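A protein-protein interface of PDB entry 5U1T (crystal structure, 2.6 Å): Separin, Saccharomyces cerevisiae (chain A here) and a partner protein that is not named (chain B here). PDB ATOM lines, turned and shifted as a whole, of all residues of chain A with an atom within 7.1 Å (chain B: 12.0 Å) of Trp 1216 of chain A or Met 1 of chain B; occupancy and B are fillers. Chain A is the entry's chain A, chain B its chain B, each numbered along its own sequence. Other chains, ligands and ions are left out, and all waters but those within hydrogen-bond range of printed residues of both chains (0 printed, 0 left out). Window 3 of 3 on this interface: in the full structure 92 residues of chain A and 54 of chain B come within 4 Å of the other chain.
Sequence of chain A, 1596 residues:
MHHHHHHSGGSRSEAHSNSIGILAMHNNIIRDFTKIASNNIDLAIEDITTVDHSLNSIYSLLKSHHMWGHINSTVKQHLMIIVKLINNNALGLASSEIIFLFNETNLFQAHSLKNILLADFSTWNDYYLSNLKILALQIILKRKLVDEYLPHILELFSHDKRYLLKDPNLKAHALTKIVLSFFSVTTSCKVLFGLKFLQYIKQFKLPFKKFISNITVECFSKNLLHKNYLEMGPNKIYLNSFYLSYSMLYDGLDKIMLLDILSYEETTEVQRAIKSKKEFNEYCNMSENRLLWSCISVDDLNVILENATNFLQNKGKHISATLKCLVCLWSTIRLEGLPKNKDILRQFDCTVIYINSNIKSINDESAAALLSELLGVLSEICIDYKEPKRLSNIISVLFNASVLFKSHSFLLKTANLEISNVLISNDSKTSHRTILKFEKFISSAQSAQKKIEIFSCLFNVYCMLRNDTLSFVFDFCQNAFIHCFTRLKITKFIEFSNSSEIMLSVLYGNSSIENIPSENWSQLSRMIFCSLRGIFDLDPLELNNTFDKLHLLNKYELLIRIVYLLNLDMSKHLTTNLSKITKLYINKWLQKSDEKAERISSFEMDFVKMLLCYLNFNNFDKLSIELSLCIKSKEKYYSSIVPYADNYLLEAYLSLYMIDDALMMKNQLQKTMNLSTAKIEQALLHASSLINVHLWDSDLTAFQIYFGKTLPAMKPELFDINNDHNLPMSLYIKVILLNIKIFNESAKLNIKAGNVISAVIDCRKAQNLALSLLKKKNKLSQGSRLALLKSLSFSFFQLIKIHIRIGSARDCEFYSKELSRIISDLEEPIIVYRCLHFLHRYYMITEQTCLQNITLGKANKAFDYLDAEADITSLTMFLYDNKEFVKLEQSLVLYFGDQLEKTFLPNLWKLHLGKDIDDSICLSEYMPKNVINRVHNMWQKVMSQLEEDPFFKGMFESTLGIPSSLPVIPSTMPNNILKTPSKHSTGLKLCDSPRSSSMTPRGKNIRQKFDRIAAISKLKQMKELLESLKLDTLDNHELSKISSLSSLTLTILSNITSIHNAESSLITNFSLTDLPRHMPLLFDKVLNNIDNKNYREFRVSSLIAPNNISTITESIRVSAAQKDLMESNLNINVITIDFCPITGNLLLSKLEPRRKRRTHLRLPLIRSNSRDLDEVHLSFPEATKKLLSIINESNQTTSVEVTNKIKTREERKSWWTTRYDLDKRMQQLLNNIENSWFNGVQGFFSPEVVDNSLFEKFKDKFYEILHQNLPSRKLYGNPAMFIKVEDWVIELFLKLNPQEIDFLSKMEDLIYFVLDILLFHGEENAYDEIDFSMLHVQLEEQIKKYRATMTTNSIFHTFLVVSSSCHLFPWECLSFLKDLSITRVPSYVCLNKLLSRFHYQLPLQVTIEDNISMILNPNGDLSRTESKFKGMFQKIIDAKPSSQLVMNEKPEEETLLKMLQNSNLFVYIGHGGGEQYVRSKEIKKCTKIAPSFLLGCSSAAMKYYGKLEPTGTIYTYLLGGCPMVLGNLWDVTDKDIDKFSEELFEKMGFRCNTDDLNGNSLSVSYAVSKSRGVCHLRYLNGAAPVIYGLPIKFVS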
ATOM      1  N   ILE A1206      29.711 -12.393  32.468  1.00  0.00           N
ATOM      2  CA  ILE A1206      29.954 -11.913  31.119  1.00  0.00           C
ATOM      3  C   ILE A1206      31.441 -11.801  30.818  1.00  0.00           C
ATOM      4  O   ILE A1206      32.139 -10.925  31.340  1.00  0.00           O
ATOM      5  CB  ILE A1206      29.316 -10.563  30.868  1.00  0.00           C
ATOM      6  CG1 ILE A1206      27.873 -10.550  31.392  1.00  0.00           C
ATOM      7  CG2 ILE A1206      29.412 -10.255  29.390  1.00  0.00           C
ATOM      8  CD1 ILE A1206      26.834 -10.171  30.354  1.00  0.00           C
ATOM      9  N   ARG A1209      33.326 -11.535  24.017  1.00  0.00           N
ATOM     10  CA  ARG A1209      32.822 -10.455  23.159  1.00  0.00           C
ATOM     11  C   ARG A1209      31.326 -10.655  22.872  1.00  0.00           C
ATOM     12  O   ARG A1209      30.567  -9.692  22.723  1.00  0.00           O
ATOM     13  CB  ARG A1209      33.623 -10.390  21.846  1.00  0.00           C
ATOM     14  CG  ARG A1209      33.290  -9.206  20.925  1.00  0.00           C
ATOM     15  CD  ARG A1209      33.839  -9.416  19.501  1.00  0.00           C
ATOM     16  NE  ARG A1209      33.753  -8.213  18.661  1.00  0.00           N
ATOM     17  CZ  ARG A1209      32.697  -7.877  17.912  1.00  0.00           C
ATOM     18  NH1 ARG A1209      31.617  -8.657  17.895  1.00  0.00           N
ATOM     19  NH2 ARG A1209      32.716  -6.758  17.181  1.00  0.00           N
ATOM     20  N   GLU A1210      30.910 -11.918  22.829  1.00  0.00           N
ATOM     21  CA  GLU A1210      29.547 -12.282  22.454  1.00  0.00           C
ATOM     22  C   GLU A1210      28.564 -12.011  23.568  1.00  0.00           C
ATOM     23  O   GLU A1210      27.465 -11.505  23.332  1.00  0.00           O
ATOM     24  CB  GLU A1210      29.478 -13.755  22.066  1.00  0.00           C
ATOM     25  CG  GLU A1210      30.235 -14.091  20.790  1.00  0.00           C
ATOM     26  CD  GLU A1210      30.212 -15.587  20.462  1.00  0.00           C
ATOM     27  OE1 GLU A1210      29.772 -16.398  21.318  1.00  0.00           O
ATOM     28  OE2 GLU A1210      30.641 -15.949  19.342  1.00  0.00           O
ATOM     29  N   GLU A1211      28.948 -12.366  24.784  1.00  0.00           N
ATOM     30  CA  GLU A1211      28.090 -12.121  25.924  1.00  0.00           C
ATOM     31  C   GLU A1211      27.967 -10.628  26.154  1.00  0.00           C
ATOM     32  O   GLU A1211      26.935 -10.145  26.590  1.00  0.00           O
ATOM     33  CB  GLU A1211      28.635 -12.822  27.157  1.00  0.00           C
ATOM     34  CG  GLU A1211      28.477 -14.314  27.073  1.00  0.00           C
ATOM     35  CD  GLU A1211      29.638 -15.083  27.675  1.00  0.00           C
ATOM     36  OE1 GLU A1211      29.458 -16.297  27.901  1.00  0.00           O
ATOM     37  OE2 GLU A1211      30.717 -14.487  27.909  1.00  0.00           O
ATOM     38  N   ARG A1212      29.036  -9.907  25.846  1.00  0.00           N
ATOM     39  CA  ARG A1212      29.045  -8.454  25.920  1.00  0.00           C
ATOM     40  C   ARG A1212      27.949  -7.841  25.050  1.00  0.00           C
ATOM     41  O   ARG A1212      27.170  -7.009  25.512  1.00  0.00           O
ATOM     42  CB  ARG A1212      30.408  -7.936  25.484  1.00  0.00           C
ATOM     43  CG  ARG A1212      31.008  -6.890  26.381  1.00  0.00           C
ATOM     44  CD  ARG A1212      32.458  -6.706  26.005  1.00  0.00           C
ATOM     45  NE  ARG A1212      33.188  -7.921  26.340  1.00  0.00           N
ATOM     46  CZ  ARG A1212      34.179  -8.436  25.623  1.00  0.00           C
ATOM     47  NH1 ARG A1212      34.572  -7.838  24.499  1.00  0.00           N
ATOM     48  NH2 ARG A1212      34.771  -9.557  26.034  1.00  0.00           N
ATOM     49  N   LYS A1213      27.891  -8.271  23.794  1.00  0.00           N
ATOM     50  CA  LYS A1213      26.957  -7.707  22.837  1.00  0.00           C
ATOM     51  C   LYS A1213      25.528  -8.100  23.175  1.00  0.00           C
ATOM     52  O   LYS A1213      24.594  -7.342  22.901  1.00  0.00           O
ATOM     53  CB  LYS A1213      27.324  -8.132  21.404  1.00  0.00           C
ATOM     54  CG  LYS A1213      28.627  -7.491  20.885  1.00  0.00           C
ATOM     55  CD  LYS A1213      28.795  -7.593  19.372  1.00  0.00           C
ATOM     56  CE  LYS A1213      29.649  -6.419  18.850  1.00  0.00           C
ATOM     57  NZ  LYS A1213      29.823  -6.331  17.348  1.00  0.00           N
ATOM     58  N   SER A1214      25.344  -9.263  23.796  1.00  0.00           N
ATOM     59  CA  SER A1214      23.994  -9.689  24.167  1.00  0.00           C
ATOM     60  C   SER A1214      23.417  -8.826  25.280  1.00  0.00           C
ATOM     61  O   SER A1214      22.272  -8.394  25.209  1.00  0.00           O
ATOM     62  CB  SER A1214      23.977 -11.157  24.585  1.00  0.00           C
ATOM     63  OG  SER A1214      23.887 -12.000  23.451  1.00  0.00           O
ATOM     64  N   TRP A1215      24.216  -8.576  26.307  1.00  0.00           N
ATOM     65  CA  TRP A1215      23.806  -7.730  27.422  1.00  0.00           C
ATOM     66  C   TRP A1215      23.444  -6.329  26.906  1.00  0.00           C
ATOM     67  O   TRP A1215      22.566  -5.663  27.447  1.00  0.00           O
ATOM     68  CB  TRP A1215      24.934  -7.687  28.465  1.00  0.00           C
ATOM     69  CG  TRP A1215      24.690  -6.909  29.728  1.00  0.00           C
ATOM     70  CD1 TRP A1215      24.200  -7.393  30.901  1.00  0.00           C
ATOM     71  CD2 TRP A1215      24.990  -5.522  29.960  1.00  0.00           C
ATOM     72  NE1 TRP A1215      24.146  -6.393  31.843  1.00  0.00           N
ATOM     73  CE2 TRP A1215      24.627  -5.235  31.291  1.00  0.00           C
ATOM     74  CE3 TRP A1215      25.521  -4.495  29.167  1.00  0.00           C
ATOM     75  CZ2 TRP A1215      24.776  -3.962  31.850  1.00  0.00           C
ATOM     76  CZ3 TRP A1215      25.665  -3.226  29.720  1.00  0.00           C
ATOM     77  CH2 TRP A1215      25.297  -2.974  31.051  1.00  0.00           C
ATOM     78  N   TRP A1216      24.106  -5.901  25.836  1.00  0.00           N
ATOM     79  CA  TRP A1216      23.878  -4.573  25.283  1.00  0.00           C
ATOM     80  C   TRP A1216      22.655  -4.548  24.374  1.00  0.00           C
ATOM     81  O   TRP A1216      21.920  -3.550  24.301  1.00  0.00           O
ATOM     82  CB  TRP A1216      25.108  -4.092  24.518  1.00  0.00           C
ATOM     83  CG  TRP A1216      26.128  -3.393  25.372  1.00  0.00           C
ATOM     84  CD1 TRP A1216      27.412  -3.781  25.588  1.00  0.00           C
ATOM     85  CD2 TRP A1216      25.944  -2.177  26.117  1.00  0.00           C
ATOM     86  NE1 TRP A1216      28.044  -2.884  26.414  1.00  0.00           N
ATOM     87  CE2 TRP A1216      27.163  -1.892  26.756  1.00  0.00           C
ATOM     88  CE3 TRP A1216      24.866  -1.303  26.303  1.00  0.00           C
ATOM     89  CZ2 TRP A1216      27.336  -0.773  27.570  1.00  0.00           C
ATOM     90  CZ3 TRP A1216      25.041  -0.197  27.115  1.00  0.00           C
ATOM     91  CH2 TRP A1216      26.265   0.058  27.736  1.00  0.00           C
ATOM     92  N   THR A1217      22.450  -5.652  23.672  1.00  0.00           N
ATOM     93  CA  THR A1217      21.252  -5.802  22.876  1.00  0.00           C
ATOM     94  C   THR A1217      20.046  -5.735  23.777  1.00  0.00           C
ATOM     95  O   THR A1217      19.085  -5.013  23.485  1.00  0.00           O
ATOM     96  CB  THR A1217      21.245  -7.118  22.120  1.00  0.00           C
ATOM     97  OG1 THR A1217      22.203  -7.049  21.058  1.00  0.00           O
ATOM     98  CG2 THR A1217      19.865  -7.385  21.547  1.00  0.00           C
ATOM     99  N   THR A1218      20.117  -6.478  24.881  1.00  0.00           N
ATOM    100  CA  THR A1218      19.015  -6.577  25.828  1.00  0.00           C
ATOM    101  C   THR A1218      18.682  -5.237  26.488  1.00  0.00           C
ATOM    102  O   THR A1218      17.505  -4.907  26.628  1.00  0.00           O
ATOM    103  CB  THR A1218      19.314  -7.638  26.934  1.00  0.00           C
ATOM    104  OG1 THR A1218      19.222  -8.960  26.379  1.00  0.00           O
ATOM    105  CG2 THR A1218      18.336  -7.518  28.099  1.00  0.00           C
ATOM    106  N   ARG A1219      19.697  -4.470  26.891  1.00  0.00           N
ATOM    107  CA  ARG A1219      19.440  -3.196  27.564  1.00  0.00           C
ATOM    108  C   ARG A1219      18.959  -2.120  26.582  1.00  0.00           C
ATOM    109  O   ARG A1219      18.079  -1.323  26.913  1.00  0.00           O
ATOM    110  CB  ARG A1219      20.675  -2.708  28.316  1.00  0.00           C
ATOM    111  CG  ARG A1219      21.138  -3.649  29.404  1.00  0.00           C
ATOM    112  CD  ARG A1219      21.872  -2.913  30.489  1.00  0.00           C
ATOM    113  NE  ARG A1219      20.960  -2.434  31.518  1.00  0.00           N
ATOM    114  CZ  ARG A1219      20.775  -1.153  31.804  1.00  0.00           C
ATOM    115  NH1 ARG A1219      21.445  -0.239  31.128  1.00  0.00           N
ATOM    116  NH2 ARG A1219      19.927  -0.785  32.762  1.00  0.00           N
ATOM    117  N   TYR A1220      19.518  -2.088  25.378  1.00  0.00           N
ATOM    118  CA  TYR A1220      19.034  -1.150  24.363  1.00  0.00           C
ATOM    119  C   TYR A1220      17.582  -1.492  24.003  1.00  0.00           C
ATOM    120  O   TYR A1220      16.781  -0.622  23.649  1.00  0.00           O
ATOM    121  CB  TYR A1220      19.925  -1.176  23.116  1.00  0.00           C
ATOM    122  CG  TYR A1220      20.979  -0.081  23.072  1.00  0.00           C
ATOM    123  CD1 TYR A1220      22.238  -0.268  23.641  1.00  0.00           C
ATOM    124  CD2 TYR A1220      20.723   1.145  22.432  1.00  0.00           C
ATOM    125  CE1 TYR A1220      23.225   0.737  23.583  1.00  0.00           C
ATOM    126  CE2 TYR A1220      21.706   2.161  22.367  1.00  0.00           C
ATOM    127  CZ  TYR A1220      22.963   1.946  22.957  1.00  0.00           C
ATOM    128  OH  TYR A1220      23.935   2.943  22.906  1.00  0.00           O
ATOM    129  N   ASP A1221      17.250  -2.769  24.120  1.00  0.00           N
ATOM    130  CA  ASP A1221      15.912  -3.247  23.827  1.00  0.00           C
ATOM    131  C   ASP A1221      14.928  -2.911  24.933  1.00  0.00           C
ATOM    132  O   ASP A1221      13.770  -2.572  24.691  1.00  0.00           O
ATOM    133  CB  ASP A1221      15.941  -4.744  23.618  1.00  0.00           C
ATOM    134  CG  ASP A1221      14.789  -5.214  22.817  1.00  0.00           C
ATOM    135  OD1 ASP A1221      13.716  -5.468  23.407  1.00  0.00           O
ATOM    136  OD2 ASP A1221      14.955  -5.292  21.583  1.00  0.00           O
ATOM    137  N   LEU A1222      15.404  -3.040  26.159  1.00  0.00           N
ATOM    138  CA  LEU A1222      14.638  -2.663  27.325  1.00  0.00           C
ATOM    139  C   LEU A1222      14.393  -1.162  27.315  1.00  0.00           C
ATOM    140  O   LEU A1222      13.324  -0.702  27.709  1.00  0.00           O
ATOM    141  CB  LEU A1222      15.371  -3.095  28.600  1.00  0.00           C
ATOM    142  CG  LEU A1222      15.237  -4.571  28.955  1.00  0.00           C
ATOM    143  CD1 LEU A1222      16.226  -4.978  30.054  1.00  0.00           C
ATOM    144  CD2 LEU A1222      13.803  -4.844  29.385  1.00  0.00           C
ATOM    145  N   THR A1533      23.192   1.706  35.687  1.00  0.00           N
ATOM    146  CA  THR A1533      24.526   1.162  35.440  1.00  0.00           C
ATOM    147  C   THR A1533      25.584   2.276  35.464  1.00  0.00           C
ATOM    148  O   THR A1533      25.292   3.426  35.123  1.00  0.00           O
ATOM    149  CB  THR A1533      24.581   0.399  34.103  1.00  0.00           C
ATOM    150  OG1 THR A1533      24.309   1.299  33.009  1.00  0.00           O
ATOM    151  CG2 THR A1533      23.571  -0.742  34.101  1.00  0.00           C
ATOM    152  N   LYS A1535      28.680   3.665  34.277  1.00  0.00           N
ATOM    153  CA  LYS A1535      29.218   4.703  33.379  1.00  0.00           C
ATOM    154  C   LYS A1535      28.193   5.789  33.058  1.00  0.00           C
ATOM    155  O   LYS A1535      28.506   6.979  33.118  1.00  0.00           O
ATOM    156  CB  LYS A1535      29.737   4.102  32.066  1.00  0.00           C
ATOM    157  CG  LYS A1535      30.959   3.235  32.230  1.00  0.00           C
ATOM    158  CD  LYS A1535      31.421   2.657  30.914  1.00  0.00           C
ATOM    159  CE  LYS A1535      32.901   2.348  31.009  1.00  0.00           C
ATOM    160  NZ  LYS A1535      33.644   3.603  31.330  1.00  0.00           N
ATOM    161  N   ASP A1536      26.973   5.376  32.725  1.00  0.00           N
ATOM    162  CA  ASP A1536      25.918   6.309  32.332  1.00  0.00           C
ATOM    163  C   ASP A1536      25.446   7.199  33.476  1.00  0.00           C
ATOM    164  O   ASP A1536      25.226   8.399  33.296  1.00  0.00           O
ATOM    165  CB  ASP A1536      24.734   5.537  31.765  1.00  0.00           C
ATOM    166  CG  ASP A1536      24.565   5.744  30.298  1.00  0.00           C
ATOM    167  OD1 ASP A1536      25.464   6.352  29.667  1.00  0.00           O
ATOM    168  OD2 ASP A1536      23.523   5.298  29.775  1.00  0.00           O
ATOM    169  N   HIS A1576      23.602   7.454  27.762  1.00  0.00           N
ATOM    170  CA  HIS A1576      23.481   6.775  26.487  1.00  0.00           C
ATOM    171  C   HIS A1576      22.151   6.080  26.411  1.00  0.00           C
ATOM    172  O   HIS A1576      21.531   6.047  25.374  1.00  0.00           O
ATOM    173  CB  HIS A1576      24.578   5.750  26.310  1.00  0.00           C
ATOM    174  CG  HIS A1576      25.766   6.268  25.576  1.00  0.00           C
ATOM    175  ND1 HIS A1576      26.923   5.539  25.432  1.00  0.00           N
ATOM    176  CD2 HIS A1576      25.976   7.440  24.943  1.00  0.00           C
ATOM    177  CE1 HIS A1576      27.794   6.241  24.738  1.00  0.00           C
ATOM    178  NE2 HIS A1576      27.243   7.399  24.428  1.00  0.00           N
ATOM    179  N   LEU A1577      21.733   5.465  27.502  1.00  0.00           N
ATOM    180  CA  LEU A1577      20.439   4.839  27.527  1.00  0.00           C
ATOM    181  C   LEU A1577      19.604   5.919  28.121  1.00  0.00           C
ATOM    182  O   LEU A1577      19.660   6.191  29.291  1.00  0.00           O
ATOM    183  CB  LEU A1577      20.441   3.588  28.367  1.00  0.00           C
ATOM    184  CG  LEU A1577      21.134   2.466  27.617  1.00  0.00           C
ATOM    185  CD1 LEU A1577      20.706   1.122  28.133  1.00  0.00           C
ATOM    186  CD2 LEU A1577      20.832   2.557  26.145  1.00  0.00           C
ATOM    187  N   ASN A1581      18.408   4.427  32.086  1.00  0.00           N
ATOM    188  CA  ASN A1581      19.235   5.182  33.020  1.00  0.00           C
ATOM    189  C   ASN A1581      18.760   6.624  33.228  1.00  0.00           C
ATOM    190  O   ASN A1581      18.566   7.052  34.374  1.00  0.00           O
ATOM    191  CB  ASN A1581      20.689   5.165  32.554  1.00  0.00           C
ATOM    192  CG  ASN A1581      21.409   3.887  32.953  1.00  0.00           C
ATOM    193  OD1 ASN A1581      21.305   3.438  34.089  1.00  0.00           O
ATOM    194  ND2 ASN A1581      22.132   3.295  32.011  1.00  0.00           N
ATOM    195  N   MET B   1      31.400  -4.401  23.095  1.00  0.00           N
ATOM    196  CA  MET B   1      31.557  -3.098  23.719  1.00  0.00           C
ATOM    197  C   MET B   1      31.507  -3.255  25.220  1.00  0.00           C
ATOM    198  O   MET B   1      30.740  -4.042  25.741  1.00  0.00           O
ATOM    199  CB  MET B   1      30.458  -2.146  23.260  1.00  0.00           C
ATOM    200  CG  MET B   1      30.549  -0.760  23.870  1.00  0.00           C
ATOM    201  SD  MET B   1      29.152   0.320  23.546  1.00  0.00           S
ATOM    202  CE  MET B   1      29.721   1.794  24.345  1.00  0.00           C
ATOM    203  N   ASP B   2      32.345  -2.521  25.923  1.00  0.00           N
ATOM    204  CA  ASP B   2      32.577  -2.841  27.307  1.00  0.00           C
ATOM    205  C   ASP B   2      31.328  -2.563  28.092  1.00  0.00           C
ATOM    206  O   ASP B   2      30.683  -1.559  27.911  1.00  0.00           O
ATOM    207  CB  ASP B   2      33.748  -2.052  27.876  1.00  0.00           C
ATOM    208  CG  ASP B   2      34.989  -2.892  28.031  1.00  0.00           C
ATOM    209  OD1 ASP B   2      36.054  -2.477  27.544  1.00  0.00           O
ATOM    210  OD2 ASP B   2      34.894  -3.971  28.638  1.00  0.00           O
ATOM    211  N   ILE B   3      31.027  -3.466  29.000  1.00  0.00           N
ATOM    212  CA  ILE B   3      29.795  -3.498  29.737  1.00  0.00           C
ATOM    213  C   ILE B   3      29.771  -2.435  30.827  1.00  0.00           C
ATOM    214  O   ILE B   3      30.799  -1.909  31.192  1.00  0.00           O
ATOM    215  CB  ILE B   3      29.680  -4.890  30.352  1.00  0.00           C
ATOM    216  CG1 ILE B   3      28.268  -5.380  30.334  1.00  0.00           C
ATOM    217  CG2 ILE B   3      30.183  -4.920  31.779  1.00  0.00           C
ATOM    218  CD1 ILE B   3      28.095  -6.550  31.261  1.00  0.00           C
ATOM    219  N   GLU B   4      28.597  -2.121  31.352  1.00  0.00           N
ATOM    220  CA  GLU B   4      28.505  -1.316  32.559  1.00  0.00           C
ATOM    221  C   GLU B   4      28.001  -2.134  33.733  1.00  0.00           C
ATOM    222  O   GLU B   4      27.569  -3.253  33.572  1.00  0.00           O
ATOM    223  CB  GLU B   4      27.590  -0.119  32.347  1.00  0.00           C
ATOM    224  CG  GLU B   4      28.022   0.855  31.272  1.00  0.00           C
ATOM    225  CD  GLU B   4      27.116   2.063  31.175  1.00  0.00           C
ATOM    226  OE1 GLU B   4      26.762   2.635  32.213  1.00  0.00           O
ATOM    227  OE2 GLU B   4      26.763   2.453  30.055  1.00  0.00           O
ATOM    228  N   ILE B   5      28.063  -1.575  34.927  1.00  0.00           N
ATOM    229  CA  ILE B   5      28.217  -2.391  36.112  1.00  0.00           C
ATOM    230  C   ILE B   5      27.427  -1.825  37.273  1.00  0.00           C
ATOM    231  O   ILE B   5      27.116  -0.658  37.296  1.00  0.00           O
ATOM    232  CB  ILE B   5      29.706  -2.524  36.472  1.00  0.00           C
ATOM    233  CG1 ILE B   5      30.059  -3.979  36.712  1.00  0.00           C
ATOM    234  CG2 ILE B   5      30.083  -1.670  37.668  1.00  0.00           C
ATOM    235  CD1 ILE B   5      31.046  -4.183  37.833  1.00  0.00           C
ATOM    236  N   ALA B   6      27.114  -2.650  38.251  1.00  0.00           N
ATOM    237  CA  ALA B   6      26.261  -2.196  39.335  1.00  0.00           C
ATOM    238  C   ALA B   6      26.769  -2.606  40.696  1.00  0.00           C
ATOM    239  O   ALA B   6      27.263  -3.695  40.865  1.00  0.00           O
ATOM    240  CB  ALA B   6      24.859  -2.720  39.126  1.00  0.00           C
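The side-chain hydroxyl of Thr 1533 of chain A is in hydrogen-bond range of the side-chain carboxylate of Glu 4 of chain B.
The backbone NH (N) of Asp 1536 of chain A lies within hydrogen-bond range of the side-chain carboxylate (OE1) of Glu 4 of chain B, at 2.8 Å.
O of Asp 2 of chain B is in hydrogen-bond range of NE1 of Trp 1216 of chain A (3.3 Å).
The indole nitrogen (NE1) of Trp 1216 of chain A lies within hydrogen-bond range of the backbone carbonyl oxygen (O) of Met 1 of chain B, 3.0 Å away.
N of Lys 1535 of chain A sits at hydrogen-bond distance from OE1 of Glu 4 of chain B, at 3.0 Å.
The side-chain carboxylate (OD2) of Asp 1536 of chain A is in hydrogen-bond range of the backbone NH (N) of Leu 1577 of chain A, 2.9 Å away.
The backbone NH (N) of His 1576 of chain A lies within hydrogen-bond range of the side-chain carboxylate (OD1) of Asp 1536 of chain A.
The backbone NH (N) of Thr 1533 of chain A sits at hydrogen-bond distance from the side-chain amide oxygen (OD1) of Asn 1581 of chain A (3.0 Å).
The side-chain carboxylate of Asp 1536 of chain A lies within hydrogen-bond range of the side-chain amide nitrogen of Asn 1581 of chain A, at 3.3 Å.
CD1 of Ile 1206 of chain A touches CD1 of Ile 3 of chain B, 3.9 Å away.
Arg 1212 of chain A touches Met 1 of chain B.
CE3 of Trp 1215 of chain A touches CG1 of Ile 3 of chain B, 3.1 Å away.
CZ2 of Trp 1215 of chain A touches O of Glu 4 of chain B, at 3.4 Å.
NE1 of Trp 1216 of chain A touches CA of Ile 3 of chain B, 3.8 Å away.
Glu 4 of chain B touches Trp 1216 of chain A.
Thr 1533 of chain A touches Ile 5 of chain B.
Trp 1216 of chain A touches just these residues of chain B: Met 1 (3.0 Å), Asp 2 (3.3 Å), Ile 3 (3.8 Å) and Glu 4 (3.4 Å).
No residue of chain B comes within 4 Å of Lys 1213 of chain A.
No residue of chain B comes within 4 Å of Ser 1214 of chain A.
Trp 1215 of chain A touches just these residues of chain B: Ile 3 (3.1 Å) and Glu 4 (3.4 Å).
No residue of chain B comes within 4 Å of Thr 1217 of chain A.
No residue of chain B comes within 4 Å of Thr 1218 of chain A.
No residue of chain B comes within 4 Å of Tyr 1220 of chain A.
No residue of chain B comes within 4 Å of His 1576 of chain A.
Printed residues of chain B within 4 Å of Lys 1535 of chain A: Glu 4.
Of the printed residues of chain B, Thr 1533 of chain A touches Glu 4 and Ile 5.
Of the printed residues of chain A, Ile 5 of chain B touches Thr 1533 (3.7 Å).
Leu 1577 of chain A touches none of the printed residues of chain B.
Asn 1581 of chain A touches none of the printed residues of chain B.
The nearest residue of chain B that does not touch Trp 1216 of chain A is Ile 5 of chain B (7.4 Å).
The nearest printed residue of chain B that does not touch Ile 1206 of chain A is Met 1 of chain B (7.3 Å).
Of the 21 printed residues of chain A, 7 touch a printed residue of chain B.
Hydrophobic or aromatic side chains of chain A that line the printed part of chain B: Ile 1206, Trp 1215 and Trp 1216.
Of the 6 printed residues of chain B, 5 touch a printed residue of chain A.
Printed residues of chain B that touch a printed residue of chain A: Met 1, Asp 2, Ile 3, Glu 4 and Ile 5.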
